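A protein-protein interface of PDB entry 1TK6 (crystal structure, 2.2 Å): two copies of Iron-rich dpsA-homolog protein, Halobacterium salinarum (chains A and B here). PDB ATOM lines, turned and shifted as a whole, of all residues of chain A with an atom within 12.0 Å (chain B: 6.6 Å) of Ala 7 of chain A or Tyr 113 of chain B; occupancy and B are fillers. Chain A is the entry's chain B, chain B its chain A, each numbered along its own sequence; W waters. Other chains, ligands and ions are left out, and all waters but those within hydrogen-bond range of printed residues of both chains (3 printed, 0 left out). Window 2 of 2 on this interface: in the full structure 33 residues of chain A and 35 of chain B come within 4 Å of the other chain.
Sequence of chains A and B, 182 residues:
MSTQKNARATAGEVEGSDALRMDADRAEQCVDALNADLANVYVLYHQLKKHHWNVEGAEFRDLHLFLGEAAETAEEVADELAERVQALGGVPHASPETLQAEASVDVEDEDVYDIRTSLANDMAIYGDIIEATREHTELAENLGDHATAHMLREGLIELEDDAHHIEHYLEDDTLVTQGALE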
ATOM      1  N   ALA A   7     -22.773 -21.475  -8.494  1.00  0.00           N
ATOM      2  CA  ALA A   7     -23.523 -22.771  -8.464  1.00  0.00           C
ATOM      3  C   ALA A   7     -23.210 -23.467  -7.176  1.00  0.00           C
ATOM      4  O   ALA A   7     -22.063 -23.469  -6.773  1.00  0.00           O
ATOM      5  CB  ALA A   7     -23.075 -23.583  -9.549  1.00  0.00           C
ATOM      6  N   ARG A   8     -24.197 -24.118  -6.560  1.00  0.00           N
ATOM      7  CA  ARG A   8     -23.932 -25.006  -5.429  1.00  0.00           C
ATOM      8  C   ARG A   8     -23.224 -26.284  -5.860  1.00  0.00           C
ATOM      9  O   ARG A   8     -22.375 -26.813  -5.135  1.00  0.00           O
ATOM     10  CB  ARG A   8     -25.252 -25.428  -4.753  1.00  0.00           C
ATOM     11  CG  ARG A   8     -25.525 -24.735  -3.605  1.00  0.00           C
ATOM     12  CD  ARG A   8     -26.876 -25.203  -2.879  1.00  0.00           C
ATOM     13  NE  ARG A   8     -26.528 -26.059  -1.756  1.00  0.00           N
ATOM     14  CZ  ARG A   8     -25.792 -25.588  -0.767  1.00  0.00           C
ATOM     15  NH1 ARG A   8     -25.448 -24.315  -0.780  1.00  0.00           N
ATOM     16  NH2 ARG A   8     -25.476 -26.367   0.258  1.00  0.00           N
ATOM     17  N   ALA A   9     -23.628 -26.830  -6.981  1.00  0.00           N
ATOM     18  CA  ALA A   9     -22.969 -27.990  -7.502  1.00  0.00           C
ATOM     19  C   ALA A   9     -22.979 -27.982  -8.973  1.00  0.00           C
ATOM     20  O   ALA A   9     -23.895 -27.511  -9.598  1.00  0.00           O
ATOM     21  CB  ALA A   9     -23.556 -29.221  -7.078  1.00  0.00           C
ATOM     22  N   THR A  10     -21.996 -28.614  -9.540  1.00  0.00           N
ATOM     23  CA  THR A  10     -21.859 -28.574 -10.942  1.00  0.00           C
ATOM     24  C   THR A  10     -22.212 -29.928 -11.553  1.00  0.00           C
ATOM     25  O   THR A  10     -21.912 -30.934 -11.034  1.00  0.00           O
ATOM     26  CB  THR A  10     -20.421 -28.016 -11.151  1.00  0.00           C
ATOM     27  OG1 THR A  10     -20.515 -26.617 -11.579  1.00  0.00           O
ATOM     28  CG2 THR A  10     -19.684 -28.680 -12.069  1.00  0.00           C
ATOM     29  N   ALA A  11     -22.949 -29.899 -12.617  1.00  0.00           N
ATOM     30  CA  ALA A  11     -23.399 -31.055 -13.322  1.00  0.00           C
ATOM     31  C   ALA A  11     -22.246 -31.923 -13.647  1.00  0.00           C
ATOM     32  O   ALA A  11     -21.270 -31.512 -14.237  1.00  0.00           O
ATOM     33  CB  ALA A  11     -24.087 -30.628 -14.618  1.00  0.00           C
ATOM     34  N   GLY A  12     -22.312 -33.162 -13.328  1.00  0.00           N
ATOM     35  CA  GLY A  12     -21.099 -33.928 -13.595  1.00  0.00           C
ATOM     36  C   GLY A  12     -20.202 -34.094 -12.400  1.00  0.00           C
ATOM     37  O   GLY A  12     -19.481 -35.087 -12.380  1.00  0.00           O
ATOM     38  N   GLU A  13     -20.209 -33.201 -11.403  1.00  0.00           N
ATOM     39  CA  GLU A  13     -19.422 -33.501 -10.212  1.00  0.00           C
ATOM     40  C   GLU A  13     -20.170 -34.516  -9.379  1.00  0.00           C
ATOM     41  O   GLU A  13     -21.408 -34.562  -9.393  1.00  0.00           O
ATOM     42  CB  GLU A  13     -19.140 -32.344  -9.207  1.00  0.00           C
ATOM     43  CG  GLU A  13     -18.813 -30.923  -9.652  1.00  0.00           C
ATOM     44  CD  GLU A  13     -18.830 -29.866  -8.491  1.00  0.00           C
ATOM     45  OE1 GLU A  13     -17.691 -29.428  -8.110  1.00  0.00           O
ATOM     46  OE2 GLU A  13     -19.946 -29.432  -8.004  1.00  0.00           O
ATOM     47  N   GLU A  15     -19.485 -35.867  -5.317  1.00  0.00           N
ATOM     48  CA  GLU A  15     -18.740 -35.650  -4.089  1.00  0.00           C
ATOM     49  C   GLU A  15     -18.836 -36.804  -3.088  1.00  0.00           C
ATOM     50  O   GLU A  15     -18.148 -36.823  -2.076  1.00  0.00           O
ATOM     51  CB  GLU A  15     -19.147 -34.340  -3.487  1.00  0.00           C
ATOM     52  CG  GLU A  15     -20.516 -34.300  -2.876  1.00  0.00           C
ATOM     53  CD  GLU A  15     -21.032 -32.860  -2.671  1.00  0.00           C
ATOM     54  OE1 GLU A  15     -20.191 -31.909  -2.885  1.00  0.00           O
ATOM     55  OE2 GLU A  15     -22.266 -32.721  -2.287  1.00  0.00           O
ATOM     56  N   GLN A  86     -28.456 -38.068  -6.213  1.00  0.00           N
ATOM     57  CA  GLN A  86     -28.196 -36.906  -5.404  1.00  0.00           C
ATOM     58  C   GLN A  86     -27.655 -37.353  -4.026  1.00  0.00           C
ATOM     59  O   GLN A  86     -26.716 -36.756  -3.479  1.00  0.00           O
ATOM     60  CB  GLN A  86     -29.419 -36.068  -5.198  1.00  0.00           C
ATOM     61  CG  GLN A  86     -29.071 -34.618  -5.102  1.00  0.00           C
ATOM     62  CD  GLN A  86     -28.919 -34.231  -3.689  1.00  0.00           C
ATOM     63  OE1 GLN A  86     -28.161 -33.360  -3.416  1.00  0.00           O
ATOM     64  NE2 GLN A  86     -29.568 -34.975  -2.766  1.00  0.00           N
ATOM     65  N   GLY A  89     -23.974 -37.683  -3.923  1.00  0.00           N
ATOM     66  CA  GLY A  89     -23.187 -36.507  -4.209  1.00  0.00           C
ATOM     67  C   GLY A  89     -23.106 -36.110  -5.670  1.00  0.00           C
ATOM     68  O   GLY A  89     -22.245 -35.319  -6.070  1.00  0.00           O
ATOM     69  N   GLY A  90     -24.014 -36.619  -6.472  1.00  0.00           N
ATOM     70  CA  GLY A  90     -24.023 -36.329  -7.886  1.00  0.00           C
ATOM     71  C   GLY A  90     -25.178 -35.398  -8.201  1.00  0.00           C
ATOM     72  O   GLY A  90     -26.018 -35.064  -7.360  1.00  0.00           O
ATOM     73  N   VAL A  91     -25.305 -35.100  -9.469  1.00  0.00           N
ATOM     74  CA  VAL A  91     -26.380 -34.238  -9.938  1.00  0.00           C
ATOM     75  C   VAL A  91     -27.219 -35.008 -10.940  1.00  0.00           C
ATOM     76  O   VAL A  91     -26.702 -35.318 -12.016  1.00  0.00           O
ATOM     77  CB  VAL A  91     -25.798 -33.115 -10.662  1.00  0.00           C
ATOM     78  CG1 VAL A  91     -26.814 -32.320 -11.335  1.00  0.00           C
ATOM     79  CG2 VAL A  91     -24.963 -32.271  -9.717  1.00  0.00           C
ATOM     80  N   PRO A  92     -28.445 -35.336 -10.645  1.00  0.00           N
ATOM     81  CA  PRO A  92     -29.258 -36.068 -11.597  1.00  0.00           C
ATOM     82  C   PRO A  92     -29.615 -35.157 -12.815  1.00  0.00           C
ATOM     83  O   PRO A  92     -29.740 -33.916 -12.711  1.00  0.00           O
ATOM     84  CB  PRO A  92     -30.515 -36.388 -10.797  1.00  0.00           C
ATOM     85  CG  PRO A  92     -30.632 -35.237  -9.930  1.00  0.00           C
ATOM     86  CD  PRO A  92     -29.173 -35.046  -9.408  1.00  0.00           C
ATOM     87  N   ALA A  94     -31.745 -33.384 -15.304  1.00  0.00           N
ATOM     88  CA  ALA A  94     -32.977 -32.791 -14.898  1.00  0.00           C
ATOM     89  C   ALA A  94     -33.798 -32.253 -16.109  1.00  0.00           C
ATOM     90  O   ALA A  94     -35.000 -32.524 -16.259  1.00  0.00           O
ATOM     91  CB  ALA A  94     -32.669 -31.699 -13.926  1.00  0.00           C
ATOM     92  N   SER A  95     -33.203 -31.489 -17.005  1.00  0.00           N
ATOM     93  CA  SER A  95     -34.104 -30.847 -17.985  1.00  0.00           C
ATOM     94  C   SER A  95     -34.505 -31.857 -18.991  1.00  0.00           C
ATOM     95  O   SER A  95     -33.850 -32.887 -19.170  1.00  0.00           O
ATOM     96  CB  SER A  95     -33.429 -29.648 -18.645  1.00  0.00           C
ATOM     97  OG  SER A  95     -32.503 -30.124 -19.588  1.00  0.00           O
ATOM     98  N   THR A  98     -31.864 -32.372 -21.667  1.00  0.00           N
ATOM     99  CA  THR A  98     -30.794 -33.169 -21.079  1.00  0.00           C
ATOM    100  C   THR A  98     -31.166 -34.626 -20.957  1.00  0.00           C
ATOM    101  O   THR A  98     -30.448 -35.462 -21.385  1.00  0.00           O
ATOM    102  CB  THR A  98     -30.423 -32.590 -19.684  1.00  0.00           C
ATOM    103  OG1 THR A  98     -30.067 -31.218 -19.831  1.00  0.00           O
ATOM    104  CG2 THR A  98     -29.187 -33.286 -19.050  1.00  0.00           C
ATOM    105  N   LYS B  50     -36.283 -31.467 -10.305  1.00  0.00           N
ATOM    106  CA  LYS B  50     -34.893 -31.120 -10.056  1.00  0.00           C
ATOM    107  C   LYS B  50     -34.752 -30.482  -8.683  1.00  0.00           C
ATOM    108  O   LYS B  50     -33.832 -30.851  -7.896  1.00  0.00           O
ATOM    109  CB  LYS B  50     -34.344 -30.165 -11.228  1.00  0.00           C
ATOM    110  CG  LYS B  50     -32.894 -29.725 -10.907  1.00  0.00           C
ATOM    111  CD  LYS B  50     -32.489 -28.505 -11.738  1.00  0.00           C
ATOM    112  CE  LYS B  50     -31.008 -28.154 -11.666  1.00  0.00           C
ATOM    113  NZ  LYS B  50     -30.733 -27.042 -12.674  1.00  0.00           N
ATOM    114  N   HIS B  51     -35.501 -29.396  -8.451  1.00  0.00           N
ATOM    115  CA  HIS B  51     -35.412 -28.735  -7.173  1.00  0.00           C
ATOM    116  C   HIS B  51     -35.868 -29.613  -5.945  1.00  0.00           C
ATOM    117  O   HIS B  51     -35.298 -29.573  -4.911  1.00  0.00           O
ATOM    118  CB  HIS B  51     -36.126 -27.372  -7.134  1.00  0.00           C
ATOM    119  CG  HIS B  51     -35.744 -26.459  -8.244  1.00  0.00           C
ATOM    120  ND1 HIS B  51     -34.732 -26.749  -9.122  1.00  0.00           N
ATOM    121  CD2 HIS B  51     -36.180 -25.223  -8.573  1.00  0.00           C
ATOM    122  CE1 HIS B  51     -34.647 -25.782 -10.023  1.00  0.00           C
ATOM    123  NE2 HIS B  51     -35.509 -24.843  -9.717  1.00  0.00           N
ATOM    124  N   ASN B  54     -32.856 -31.843  -5.270  1.00  0.00           N
ATOM    125  CA  ASN B  54     -31.572 -31.320  -4.910  1.00  0.00           C
ATOM    126  C   ASN B  54     -31.650 -30.430  -3.666  1.00  0.00           C
ATOM    127  O   ASN B  54     -30.633 -30.017  -3.119  1.00  0.00           O
ATOM    128  CB  ASN B  54     -30.934 -30.555  -6.072  1.00  0.00           C
ATOM    129  CG  ASN B  54     -30.397 -31.431  -7.226  1.00  0.00           C
ATOM    130  OD1 ASN B  54     -29.515 -32.134  -7.064  1.00  0.00           O
ATOM    131  ND2 ASN B  54     -30.841 -31.174  -8.433  1.00  0.00           N
ATOM    132  N   GLU B 108     -33.511 -23.765 -16.344  1.00  0.00           N
ATOM    133  CA  GLU B 108     -32.193 -23.719 -15.766  1.00  0.00           C
ATOM    134  C   GLU B 108     -31.247 -24.578 -16.552  1.00  0.00           C
ATOM    135  O   GLU B 108     -31.664 -25.607 -17.032  1.00  0.00           O
ATOM    136  CB  GLU B 108     -32.226 -24.248 -14.333  1.00  0.00           C
ATOM    137  CG  GLU B 108     -32.484 -23.169 -13.311  1.00  0.00           C
ATOM    138  CD  GLU B 108     -32.534 -23.723 -11.859  1.00  0.00           C
ATOM    139  OE1 GLU B 108     -32.821 -22.880 -11.000  1.00  0.00           O
ATOM    140  OE2 GLU B 108     -32.113 -24.891 -11.562  1.00  0.00           O
ATOM    141  N   ASP B 109     -29.959 -24.213 -16.602  1.00  0.00           N
ATOM    142  CA  ASP B 109     -28.942 -25.180 -17.083  1.00  0.00           C
ATOM    143  C   ASP B 109     -28.816 -26.286 -16.042  1.00  0.00           C
ATOM    144  O   ASP B 109     -29.471 -26.199 -14.986  1.00  0.00           O
ATOM    145  CB  ASP B 109     -27.625 -24.486 -17.414  1.00  0.00           C
ATOM    146  CG  ASP B 109     -26.960 -23.863 -16.224  1.00  0.00           C
ATOM    147  OD1 ASP B 109     -26.115 -22.944 -16.475  1.00  0.00           O
ATOM    148  OD2 ASP B 109     -27.203 -24.151 -15.028  1.00  0.00           O
ATOM    149  N   GLU B 110     -27.908 -27.216 -16.263  1.00  0.00           N
ATOM    150  CA  GLU B 110     -27.827 -28.414 -15.496  1.00  0.00           C
ATOM    151  C   GLU B 110     -27.164 -28.294 -14.150  1.00  0.00           C
ATOM    152  O   GLU B 110     -27.140 -29.214 -13.382  1.00  0.00           O
ATOM    153  CB  GLU B 110     -27.260 -29.503 -16.404  1.00  0.00           C
ATOM    154  CG  GLU B 110     -28.345 -29.879 -17.433  1.00  0.00           C
ATOM    155  CD  GLU B 110     -29.635 -30.490 -16.754  1.00  0.00           C
ATOM    156  OE1 GLU B 110     -30.761 -30.153 -17.221  1.00  0.00           O
ATOM    157  OE2 GLU B 110     -29.537 -31.317 -15.765  1.00  0.00           O
ATOM    158  N   ASP B 111     -26.585 -27.162 -13.850  1.00  0.00           N
ATOM    159  CA  ASP B 111     -25.973 -26.993 -12.588  1.00  0.00           C
ATOM    160  C   ASP B 111     -27.073 -26.870 -11.570  1.00  0.00           C
ATOM    161  O   ASP B 111     -28.258 -26.590 -11.918  1.00  0.00           O
ATOM    162  CB  ASP B 111     -25.060 -25.750 -12.609  1.00  0.00           C
ATOM    163  CG  ASP B 111     -23.726 -26.008 -13.408  1.00  0.00           C
ATOM    164  OD1 ASP B 111     -23.309 -27.202 -13.598  1.00  0.00           O
ATOM    165  OD2 ASP B 111     -23.066 -25.070 -13.934  1.00  0.00           O
ATOM    166  N   VAL B 112     -26.696 -27.029 -10.299  1.00  0.00           N
ATOM    167  CA  VAL B 112     -27.645 -26.900  -9.162  1.00  0.00           C
ATOM    168  C   VAL B 112     -27.350 -25.546  -8.422  1.00  0.00           C
ATOM    169  O   VAL B 112     -26.251 -25.286  -8.026  1.00  0.00           O
ATOM    170  CB  VAL B 112     -27.448 -28.048  -8.228  1.00  0.00           C
ATOM    171  CG1 VAL B 112     -28.310 -27.931  -6.911  1.00  0.00           C
ATOM    172  CG2 VAL B 112     -27.717 -29.297  -8.934  1.00  0.00           C
ATOM    173  N   TYR B 113     -28.363 -24.732  -8.236  1.00  0.00           N
ATOM    174  CA  TYR B 113     -28.195 -23.487  -7.582  1.00  0.00           C
ATOM    175  C   TYR B 113     -28.797 -23.626  -6.205  1.00  0.00           C
ATOM    176  O   TYR B 113     -29.533 -24.563  -5.915  1.00  0.00           O
ATOM    177  CB  TYR B 113     -28.871 -22.362  -8.398  1.00  0.00           C
ATOM    178  CG  TYR B 113     -28.225 -22.307  -9.736  1.00  0.00           C
ATOM    179  CD1 TYR B 113     -28.715 -23.045 -10.811  1.00  0.00           C
ATOM    180  CD2 TYR B 113     -27.034 -21.606  -9.906  1.00  0.00           C
ATOM    181  CE1 TYR B 113     -28.046 -23.036 -12.052  1.00  0.00           C
ATOM    182  CE2 TYR B 113     -26.359 -21.623 -11.092  1.00  0.00           C
ATOM    183  CZ  TYR B 113     -26.866 -22.378 -12.154  1.00  0.00           C
ATOM    184  OH  TYR B 113     -26.172 -22.404 -13.303  1.00  0.00           O
ATOM    185  N   ASP B 114     -28.562 -22.628  -5.419  1.00  0.00           N
ATOM    186  CA  ASP B 114     -29.099 -22.505  -4.135  1.00  0.00           C
ATOM    187  C   ASP B 114     -30.601 -22.368  -4.166  1.00  0.00           C
ATOM    188  O   ASP B 114     -31.185 -22.158  -5.201  1.00  0.00           O
ATOM    189  CB  ASP B 114     -28.440 -21.347  -3.300  1.00  0.00           C
ATOM    190  CG  ASP B 114     -28.839 -19.921  -3.738  1.00  0.00           C
ATOM    191  OD1 ASP B 114     -28.032 -18.978  -3.460  1.00  0.00           O
ATOM    192  OD2 ASP B 114     -29.866 -19.594  -4.318  1.00  0.00           O
ATOM    193  N   ILE B 115     -31.206 -22.586  -3.005  1.00  0.00           N
ATOM    194  CA  ILE B 115     -32.627 -22.774  -2.969  1.00  0.00           C
ATOM    195  C   ILE B 115     -33.421 -21.477  -3.339  1.00  0.00           C
ATOM    196  O   ILE B 115     -34.382 -21.484  -4.121  1.00  0.00           O
ATOM    197  CB  ILE B 115     -33.023 -23.423  -1.703  1.00  0.00           C
ATOM    198  CG1 ILE B 115     -34.486 -23.786  -1.766  1.00  0.00           C
ATOM    199  CG2 ILE B 115     -32.885 -22.533  -0.524  1.00  0.00           C
ATOM    200  CD1 ILE B 115     -34.850 -24.656  -2.969  1.00  0.00           C
ATOM    201  N   ARG B 116     -32.938 -20.352  -2.911  1.00  0.00           N
ATOM    202  CA  ARG B 116     -33.624 -19.070  -3.288  1.00  0.00           C
ATOM    203  C   ARG B 116     -33.583 -18.864  -4.787  1.00  0.00           C
ATOM    204  O   ARG B 116     -34.637 -18.624  -5.378  1.00  0.00           O
ATOM    205  CB  ARG B 116     -33.008 -17.859  -2.603  1.00  0.00           C
ATOM    206  CG  ARG B 116     -33.185 -17.853  -1.086  1.00  0.00           C
ATOM    207  CD  ARG B 116     -32.824 -16.590  -0.404  1.00  0.00           C
ATOM    208  NE  ARG B 116     -33.686 -15.544  -0.856  1.00  0.00           N
ATOM    209  CZ  ARG B 116     -34.874 -15.244  -0.350  1.00  0.00           C
ATOM    210  NH1 ARG B 116     -35.443 -15.893   0.631  1.00  0.00           N
ATOM    211  NH2 ARG B 116     -35.554 -14.298  -0.945  1.00  0.00           N
ATOM    212  N   THR B 117     -32.415 -19.084  -5.419  1.00  0.00           N
ATOM    213  CA  THR B 117     -32.315 -18.911  -6.853  1.00  0.00           C
ATOM    214  C   THR B 117     -33.187 -19.852  -7.582  1.00  0.00           C
ATOM    215  O   THR B 117     -33.871 -19.473  -8.539  1.00  0.00           O
ATOM    216  CB  THR B 117     -30.859 -19.183  -7.294  1.00  0.00           C
ATOM    217  OG1 THR B 117     -29.986 -18.189  -6.724  1.00  0.00           O
ATOM    218  CG2 THR B 117     -30.719 -19.067  -8.812  1.00  0.00           C
ATOM    219  N   SER B 118     -33.204 -21.109  -7.143  1.00  0.00           N
ATOM    220  CA  SER B 118     -33.980 -22.123  -7.817  1.00  0.00           C
ATOM    221  C   SER B 118     -35.469 -21.763  -7.699  1.00  0.00           C
ATOM    222  O   SER B 118     -36.193 -21.902  -8.657  1.00  0.00           O
ATOM    223  CB  SER B 118     -33.756 -23.478  -7.179  1.00  0.00           C
ATOM    224  OG  SER B 118     -32.423 -23.931  -7.105  1.00  0.00           O
ATOM    225  N   ASN B 121     -36.448 -18.902 -10.042  1.00  0.00           N
ATOM    226  CA  ASN B 121     -36.591 -19.408 -11.369  1.00  0.00           C
ATOM    227  C   ASN B 121     -37.916 -20.146 -11.532  1.00  0.00           C
ATOM    228  O   ASN B 121     -38.579 -20.048 -12.557  1.00  0.00           O
ATOM    229  CB  ASN B 121     -35.458 -20.353 -11.618  1.00  0.00           C
ATOM    230  CG  ASN B 121     -34.152 -19.638 -11.837  1.00  0.00           C
ATOM    231  OD1 ASN B 121     -34.167 -18.519 -12.231  1.00  0.00           O
ATOM    232  ND2 ASN B 121     -33.051 -20.318 -11.649  1.00  0.00           N
HETATM  233  O   HOH W   1     -28.399 -28.277  -2.932  1.00  0.00           O
HETATM  234  O   HOH W   2     -30.254 -31.991 -11.141  1.00  0.00           O
HETATM  235  O   HOH W   3     -29.401 -30.493 -13.269  1.00  0.00           O
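Among the printed residues, pairs that only touch across the chains: Ala 7 of chain A with Val 112 of chain B, Ala 7 of chain A with Tyr 113 of chain B, Arg 8 of chain A with Asp 114 of chain B, Ala 9 of chain A with Asp 111 of chain B, Ala 11 of chain A with Glu 110 of chain B, Gln 86 of chain A with Asn 54 of chain B, Val 91 of chain A with Glu 110 of chain B, Val 91 of chain A with Val 112 of chain B, Pro 92 of chain A with Asn 54 of chain B and Ala 94 of chain A with Lys 50 of chain B.
The side-chain carboxylate (OE2) of Glu 110 of chain B sits at hydrogen-bond distance from the backbone NH (N) of Ala 94 of chain A.
The side-chain carboxylate of Glu 110 of chain B sits at hydrogen-bond distance from the backbone NH of Ser 95 of chain A (2.8 Å).
The side-chain carboxylate (OE1) of Glu 110 of chain B sits at hydrogen-bond distance from the side-chain hydroxyl (OG1) of Thr 98 of chain A (2.9 Å).
OD1 of Asp 111 of chain B sits close to OG1 of Thr 10 of chain A, at 3.5 Å.
OD1 of Asp 111 of chain B is in hydrogen-bond range of N of Ala 11 of chain A.
The backbone NH (N) of Arg 8 of chain A is in hydrogen-bond range of the backbone carbonyl oxygen (O) of Val 112 of chain B.
The backbone NH of Val 112 of chain B is in hydrogen-bond range of the backbone carbonyl oxygen of Ala 9 of chain A, 2.9 Å away.
Of the 16 printed residues of chain A, 11 touch a printed residue of chain B.
Hydrophobic or aromatic side chains of chain A that line the printed part of chain B: Ala 7, Ala 11, Val 91, Pro 92 and Ala 94.
Of the 15 printed residues of chain B, 7 touch a printed residue of chain A.
Printed residues of chain B that touch a printed residue of chain A: Lys 50, Asn 54, Glu 110, Asp 111, Val 112, Tyr 113 and Asp 114.
Hydrophobic or aromatic side chains of chain B that line the printed part of chain A: Val 112 and Tyr 113.
Among the printed residues, no Asp or Glu carboxylate lies within 4 Å of a Lys or Arg side-chain nitrogen of the other chain.
NZ of Lys 50 of chain B lies within hydrogen-bond range of O of Asp 109 of chain B, at 2.8 Å.
The side-chain amino group (NZ) of Lys 50 of chain B is in hydrogen-bond range of the backbone carbonyl oxygen (O) of Asp 111 of chain B.
The backbone carbonyl oxygen of Tyr 113 of chain B lies within hydrogen-bond range of the side-chain hydroxyl of Ser 118 of chain B, at 3.2 Å.
N of Arg 116 of chain B lies close to OD2 of Asp 114 of chain B, 3.5 Å away.
N of Thr 10 of chain A lies within hydrogen-bond range of OE2 of Glu 13 of chain A, at 2.7 Å.
OG of Ser 95 of chain A sits at hydrogen-bond distance from OG1 of Thr 98 of chain A (2.7 Å).
Of the printed residues of chain B, Ala 7 of chain A touches Val 112 (3.6 Å) and Tyr 113 (3.97 Å).
No residue of chain A comes within 4 Å of Asp 109 of chain B.
Of chain A, only Ala 9, Thr 10 and Ala 11 come within 4 Å of Asp 111 of chain B.
Of the printed residues of chain A, Val 112 of chain B touches Ala 7 (3.6 Å), Arg 8 (2.8 Å), Ala 9 (2.9 Å) and Val 91 (3.96 Å).
Of the printed residues of chain A, Asp 114 of chain B touches Arg 8.
No residue of chain A comes within 4 Å of Ile 115 of chain B.
No residue of chain A comes within 4 Å of Thr 117 of chain B.
No residue of chain A comes within 4 Å of Ser 118 of chain B.
Printed residues of chain B within 4 Å of Ala 94 of chain A: Lys 50 and Glu 110.
Of the printed residues of chain B, Thr 10 of chain A touches Asp 111.
Of the printed residues of chain B, Gln 86 of chain A touches Asn 54.
Printed residues of chain A within 4 Å of Asn 54 of chain B: Gln 86 and Pro 92.
Glu 13 of chain A touches none of the printed residues of chain B.
The nearest printed residue of chain B that does not touch Ser 95 of chain A is Glu 108 of chain B (4.7 Å).
Water W2 bridges the backbone carbonyl oxygen of Pro 92 of chain A and the side-chain amide nitrogen of Asn 54 of chain B.
Water W3 lies within hydrogen-bond range of O of Glu 110 of chain B (2.6 Å) and O of Pro 92 of chain A (3.5 Å).
Water W1 lies within hydrogen-bond range of O of Asn 54 of chain B and NE of Arg 8 of chain A.
No position is printed for both chains.
Of the 17 pairs that touch across the chains among the printed residues, none has its exchanged pair printed and touching as well.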
